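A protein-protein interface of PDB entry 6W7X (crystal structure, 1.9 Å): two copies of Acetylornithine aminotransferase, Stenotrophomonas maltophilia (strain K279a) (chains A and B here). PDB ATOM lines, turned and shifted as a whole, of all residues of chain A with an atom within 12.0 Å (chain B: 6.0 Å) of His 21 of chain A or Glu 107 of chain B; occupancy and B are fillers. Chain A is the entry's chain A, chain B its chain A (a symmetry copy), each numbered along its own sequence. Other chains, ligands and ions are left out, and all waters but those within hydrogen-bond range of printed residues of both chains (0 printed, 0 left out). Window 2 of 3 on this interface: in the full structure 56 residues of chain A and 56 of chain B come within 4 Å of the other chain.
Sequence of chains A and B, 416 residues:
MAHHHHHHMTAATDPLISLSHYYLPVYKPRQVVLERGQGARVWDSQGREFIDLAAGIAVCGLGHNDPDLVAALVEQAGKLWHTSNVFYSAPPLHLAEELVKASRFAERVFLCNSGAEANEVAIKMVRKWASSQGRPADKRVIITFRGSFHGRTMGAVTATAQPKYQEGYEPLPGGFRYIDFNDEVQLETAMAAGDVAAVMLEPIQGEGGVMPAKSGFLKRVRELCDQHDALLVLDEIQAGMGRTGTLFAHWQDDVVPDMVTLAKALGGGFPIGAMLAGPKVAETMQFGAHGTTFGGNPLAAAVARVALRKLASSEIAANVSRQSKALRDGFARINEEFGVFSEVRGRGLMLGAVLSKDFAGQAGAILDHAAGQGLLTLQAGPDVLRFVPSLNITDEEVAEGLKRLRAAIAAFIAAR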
ATOM      1  N   LEU A  16      13.866   0.587  14.125  1.00  0.00           N
ATOM      2  CA  LEU A  16      13.590  -0.730  14.690  1.00  0.00           C
ATOM      3  C   LEU A  16      13.482  -0.659  16.213  1.00  0.00           C
ATOM      4  O   LEU A  16      12.722  -1.410  16.822  1.00  0.00           O
ATOM      5  CB  LEU A  16      14.673  -1.733  14.277  1.00  0.00           C
ATOM      6  N   ILE A  17      14.242   0.257  16.826  1.00  0.00           N
ATOM      7  CA  ILE A  17      14.161   0.474  18.268  1.00  0.00           C
ATOM      8  C   ILE A  17      13.072   1.476  18.640  1.00  0.00           C
ATOM      9  O   ILE A  17      12.938   1.816  19.824  1.00  0.00           O
ATOM     10  CB  ILE A  17      15.512   0.957  18.838  1.00  0.00           C
ATOM     11  N   SER A  18      12.290   1.963  17.668  1.00  0.00           N
ATOM     12  CA  SER A  18      11.206   2.901  17.943  1.00  0.00           C
ATOM     13  C   SER A  18       9.934   2.213  18.418  1.00  0.00           C
ATOM     14  O   SER A  18       9.009   2.901  18.866  1.00  0.00           O
ATOM     15  CB  SER A  18      10.885   3.725  16.699  1.00  0.00           C
ATOM     16  OG  SER A  18       9.933   3.052  15.889  1.00  0.00           O
ATOM     17  N   LEU A  19       9.855   0.887  18.301  1.00  0.00           N
ATOM     18  CA  LEU A  19       8.750   0.113  18.851  1.00  0.00           C
ATOM     19  C   LEU A  19       8.924  -0.177  20.339  1.00  0.00           C
ATOM     20  O   LEU A  19       8.149  -0.960  20.898  1.00  0.00           O
ATOM     21  CB  LEU A  19       8.584  -1.198  18.074  1.00  0.00           C
ATOM     22  N   SER A  20       9.927   0.431  20.984  1.00  0.00           N
ATOM     23  CA  SER A  20      10.073   0.362  22.431  1.00  0.00           C
ATOM     24  C   SER A  20       9.139   1.320  23.161  1.00  0.00           C
ATOM     25  O   SER A  20       9.097   1.294  24.397  1.00  0.00           O
ATOM     26  CB  SER A  20      11.522   0.653  22.833  1.00  0.00           C
ATOM     27  OG  SER A  20      11.677   0.593  24.241  1.00  0.00           O
ATOM     28  N   HIS A  21       8.404   2.168  22.429  1.00  0.00           N
ATOM     29  CA  HIS A  21       7.309   2.953  22.986  1.00  0.00           C
ATOM     30  C   HIS A  21       6.100   2.092  23.326  1.00  0.00           C
ATOM     31  O   HIS A  21       5.109   2.611  23.858  1.00  0.00           O
ATOM     32  CB  HIS A  21       6.908   4.064  22.010  1.00  0.00           C
ATOM     33  N   TYR A  22       6.165   0.797  23.013  1.00  0.00           N
ATOM     34  CA  TYR A  22       5.165  -0.187  23.408  1.00  0.00           C
ATOM     35  C   TYR A  22       5.626  -1.065  24.565  1.00  0.00           C
ATOM     36  O   TYR A  22       4.785  -1.573  25.313  1.00  0.00           O
ATOM     37  CB  TYR A  22       4.798  -1.082  22.216  1.00  0.00           C
ATOM     38  CG  TYR A  22       4.363  -0.336  20.969  1.00  0.00           C
ATOM     39  CD1 TYR A  22       3.029  -0.024  20.753  1.00  0.00           C
ATOM     40  CD2 TYR A  22       5.288   0.045  19.999  1.00  0.00           C
ATOM     41  CE1 TYR A  22       2.629   0.647  19.618  1.00  0.00           C
ATOM     42  CE2 TYR A  22       4.891   0.724  18.855  1.00  0.00           C
ATOM     43  CZ  TYR A  22       3.564   1.019  18.671  1.00  0.00           C
ATOM     44  OH  TYR A  22       3.158   1.696  17.538  1.00  0.00           O
ATOM     45  N   TYR A  23       6.936  -1.253  24.732  1.00  0.00           N
ATOM     46  CA  TYR A  23       7.476  -2.113  25.787  1.00  0.00           C
ATOM     47  C   TYR A  23       7.747  -1.322  27.066  1.00  0.00           C
ATOM     48  O   TYR A  23       6.935  -0.487  27.473  1.00  0.00           O
ATOM     49  CB  TYR A  23       8.760  -2.805  25.317  1.00  0.00           C
ATOM     50  N   PRO A  29      17.645   0.436  29.234  1.00  0.00           N
ATOM     51  CA  PRO A  29      18.286  -0.557  28.365  1.00  0.00           C
ATOM     52  C   PRO A  29      19.230   0.088  27.355  1.00  0.00           C
ATOM     53  O   PRO A  29      18.895   1.133  26.792  1.00  0.00           O
ATOM     54  CB  PRO A  29      17.102  -1.224  27.650  1.00  0.00           C
ATOM     55  CG  PRO A  29      15.896  -0.889  28.486  1.00  0.00           C
ATOM     56  CD  PRO A  29      16.182   0.456  29.068  1.00  0.00           C
ATOM     57  N   GLN A  31      20.863   1.033  24.010  1.00  0.00           N
ATOM     58  CA  GLN A  31      20.262   1.175  22.683  1.00  0.00           C
ATOM     59  C   GLN A  31      21.055   0.356  21.661  1.00  0.00           C
ATOM     60  O   GLN A  31      21.690   0.879  20.743  1.00  0.00           O
ATOM     61  CB  GLN A  31      20.191   2.643  22.287  1.00  0.00           C
ATOM     62  N   VAL A  33      20.360  -3.359  19.490  1.00  0.00           N
ATOM     63  CA  VAL A  33      19.478  -4.465  19.131  1.00  0.00           C
ATOM     64  C   VAL A  33      20.339  -5.646  18.697  1.00  0.00           C
ATOM     65  O   VAL A  33      20.985  -5.609  17.644  1.00  0.00           O
ATOM     66  CB  VAL A  33      18.497  -4.072  18.024  1.00  0.00           C
ATOM     67  CG1 VAL A  33      17.550  -5.226  17.748  1.00  0.00           C
ATOM     68  CG2 VAL A  33      17.732  -2.800  18.400  1.00  0.00           C
ATOM     69  N   VAL B 100       0.005  -4.862  21.155  1.00  0.00           N
ATOM     70  CA  VAL B 100      -0.670  -3.613  21.507  1.00  0.00           C
ATOM     71  C   VAL B 100      -1.706  -3.262  20.453  1.00  0.00           C
ATOM     72  O   VAL B 100      -2.853  -2.923  20.769  1.00  0.00           O
ATOM     73  CB  VAL B 100       0.353  -2.477  21.696  1.00  0.00           C
ATOM     74  CG1 VAL B 100      -0.345  -1.142  21.678  1.00  0.00           C
ATOM     75  CG2 VAL B 100       1.079  -2.659  23.010  1.00  0.00           C
ATOM     76  N   SER B 103      -4.821  -5.610  20.434  1.00  0.00           N
ATOM     77  CA  SER B 103      -5.675  -5.568  21.617  1.00  0.00           C
ATOM     78  C   SER B 103      -6.829  -4.585  21.475  1.00  0.00           C
ATOM     79  O   SER B 103      -7.849  -4.742  22.155  1.00  0.00           O
ATOM     80  CB  SER B 103      -4.856  -5.179  22.842  1.00  0.00           C
ATOM     81  OG  SER B 103      -4.492  -3.810  22.760  1.00  0.00           O
ATOM     82  N   PHE B 105      -6.972  -1.650  22.652  1.00  0.00           N
ATOM     83  CA  PHE B 105      -7.123  -0.736  23.784  1.00  0.00           C
ATOM     84  C   PHE B 105      -5.776  -0.329  24.366  1.00  0.00           C
ATOM     85  O   PHE B 105      -5.626   0.772  24.904  1.00  0.00           O
ATOM     86  CB  PHE B 105      -7.975  -1.370  24.888  1.00  0.00           C
ATOM     87  CG  PHE B 105      -7.197  -2.306  25.790  1.00  0.00           C
ATOM     88  CD1 PHE B 105      -7.026  -3.624  25.435  1.00  0.00           C
ATOM     89  CD2 PHE B 105      -6.638  -1.853  26.977  1.00  0.00           C
ATOM     90  CE1 PHE B 105      -6.305  -4.492  26.245  1.00  0.00           C
ATOM     91  CE2 PHE B 105      -5.905  -2.707  27.799  1.00  0.00           C
ATOM     92  CZ  PHE B 105      -5.739  -4.030  27.432  1.00  0.00           C
ATOM     93  N   ALA B 106      -4.797  -1.222  24.284  1.00  0.00           N
ATOM     94  CA  ALA B 106      -3.589  -1.078  25.067  1.00  0.00           C
ATOM     95  C   ALA B 106      -2.669  -0.027  24.468  1.00  0.00           C
ATOM     96  O   ALA B 106      -2.678   0.222  23.261  1.00  0.00           O
ATOM     97  CB  ALA B 106      -2.864  -2.416  25.159  1.00  0.00           C
ATOM     98  N   GLU B 107      -1.875   0.600  25.338  1.00  0.00           N
ATOM     99  CA  GLU B 107      -0.793   1.480  24.920  1.00  0.00           C
ATOM    100  C   GLU B 107       0.581   0.896  25.200  1.00  0.00           C
ATOM    101  O   GLU B 107       1.537   1.222  24.494  1.00  0.00           O
ATOM    102  CB  GLU B 107      -0.904   2.839  25.621  1.00  0.00           C
ATOM    103  CG  GLU B 107      -1.705   3.867  24.838  1.00  0.00           C
ATOM    104  CD  GLU B 107      -1.875   5.174  25.582  1.00  0.00           C
ATOM    105  OE1 GLU B 107      -1.038   5.484  26.456  1.00  0.00           O
ATOM    106  OE2 GLU B 107      -2.856   5.889  25.291  1.00  0.00           O
ATOM    107  N   ARG B 108       0.691   0.032  26.203  1.00  0.00           N
ATOM    108  CA  ARG B 108       1.961  -0.563  26.578  1.00  0.00           C
ATOM    109  C   ARG B 108       1.726  -2.025  26.921  1.00  0.00           C
ATOM    110  O   ARG B 108       0.619  -2.430  27.290  1.00  0.00           O
ATOM    111  CB  ARG B 108       2.601   0.187  27.755  1.00  0.00           C
ATOM    112  N   VAL B 109       2.777  -2.826  26.775  1.00  0.00           N
ATOM    113  CA  VAL B 109       2.730  -4.237  27.131  1.00  0.00           C
ATOM    114  C   VAL B 109       3.968  -4.570  27.946  1.00  0.00           C
ATOM    115  O   VAL B 109       5.071  -4.102  27.645  1.00  0.00           O
ATOM    116  CB  VAL B 109       2.638  -5.155  25.896  1.00  0.00           C
ATOM    117  CG1 VAL B 109       3.823  -4.950  24.999  1.00  0.00           C
ATOM    118  CG2 VAL B 109       2.552  -6.614  26.325  1.00  0.00           C
ATOM    119  N   ALA B 277      -1.567  -2.927  28.970  1.00  0.00           N
ATOM    120  CA  ALA B 277      -1.955  -1.765  29.763  1.00  0.00           C
ATOM    121  C   ALA B 277      -2.560  -0.681  28.883  1.00  0.00           C
ATOM    122  O   ALA B 277      -1.929  -0.232  27.917  1.00  0.00           O
ATOM    123  CB  ALA B 277      -0.756  -1.189  30.516  1.00  0.00           C
ATOM    124  N   GLY B 278      -3.767  -0.227  29.250  1.00  0.00           N
ATOM    125  CA  GLY B 278      -4.387   0.891  28.586  1.00  0.00           C
ATOM    126  C   GLY B 278      -3.868   2.226  29.081  1.00  0.00           C
ATOM    127  O   GLY B 278      -3.001   2.316  29.960  1.00  0.00           O
ATOM    128  N   PRO B 279      -4.427   3.301  28.513  1.00  0.00           N
ATOM    129  CA  PRO B 279      -3.915   4.653  28.801  1.00  0.00           C
ATOM    130  C   PRO B 279      -3.932   5.053  30.267  1.00  0.00           C
ATOM    131  O   PRO B 279      -3.060   5.824  30.688  1.00  0.00           O
ATOM    132  CB  PRO B 279      -4.849   5.559  27.980  1.00  0.00           C
ATOM    133  CG  PRO B 279      -5.386   4.680  26.908  1.00  0.00           C
ATOM    134  CD  PRO B 279      -5.496   3.314  27.495  1.00  0.00           C
ATOM    135  N   ALA B 282      -0.757   3.088  31.555  1.00  0.00           N
ATOM    136  CA  ALA B 282       0.477   3.089  30.784  1.00  0.00           C
ATOM    137  C   ALA B 282       1.426   4.193  31.231  1.00  0.00           C
ATOM    138  O   ALA B 282       2.642   4.063  31.047  1.00  0.00           O
ATOM    139  CB  ALA B 282       0.165   3.230  29.294  1.00  0.00           C
ATOM    140  N   GLU B 283       0.900   5.270  31.820  1.00  0.00           N
ATOM    141  CA  GLU B 283       1.711   6.345  32.374  1.00  0.00           C
ATOM    142  C   GLU B 283       2.209   6.044  33.783  1.00  0.00           C
ATOM    143  O   GLU B 283       2.635   6.964  34.490  1.00  0.00           O
ATOM    144  CB  GLU B 283       0.918   7.653  32.371  1.00  0.00           C
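Among the printed residues, pairs that only touch across the chains: Tyr 22 of chain A with Arg 108 of chain B (3.3 Å), Tyr 23 of chain A with Val 109 of chain B (3.6 Å), Tyr 22 of chain A with Val 100 of chain B (3.7 Å) and His 21 of chain A with Glu 107 of chain B (3.9 Å).
No position is printed for both chains.
The backbone carbonyl oxygen (O) of Tyr 22 of chain A lies within hydrogen-bond range of the backbone NH (N) of Val 109 of chain B (2.8 Å).
Of the 12 printed residues of chain B, 4 touch a printed residue of chain A. Printed residues of chain B that touch a printed residue of chain A: Val 100, Glu 107, Arg 108 and Val 109. Among the printed residues, 5 pairs touch across the chains.
The side-chain hydroxyl (OG) of Ser 103 of chain B is in hydrogen-bond range of the backbone carbonyl oxygen (O) of Val 100 of chain B (2.7 Å). O of Ala 277 of chain B is in hydrogen-bond range of N of Glu 107 of chain B (2.7 Å). N of Ala 277 of chain B lies within hydrogen-bond range of O of Arg 108 of chain B, 2.8 Å away.
Printed residues of chain B within 4 Å of His 21 of chain A: Glu 107. Val 100 of chain B touches just one residue of chain A: Tyr 22 (3.7 Å). No residue of chain A comes within 4 Å of Phe 105 of chain B. Printed residues of chain A within 4 Å of Arg 108 of chain B: Tyr 22 (3.3 Å). Val 109 of chain B touches just these residues of chain A: Tyr 22 (2.8 Å) and Tyr 23 (3.6 Å). No residue of chain A comes within 4 Å of Gly 278 of chain B. No residue of chain A comes within 4 Å of Pro 279 of chain B. No residue of chain A comes within 4 Å of Ala 282 of chain B. Of the printed residues of chain B, Tyr 23 of chain A touches Val 109. Of the printed residues of chain B, Tyr 22 of chain A touches Val 100 (3.7 Å), Arg 108 (3.3 Å) and Val 109 (2.8 Å). Glu 283 of chain B touches none of the printed residues of chain A. Ser 103 of chain B touches none of the printed residues of chain A. The nearest residue of chain B that does not touch His 21 of chain A is Arg 108 of chain B (5.2 Å). The nearest residue of chain A that does not touch Glu 107 of chain B is Tyr 22 of chain A (4.04 Å).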
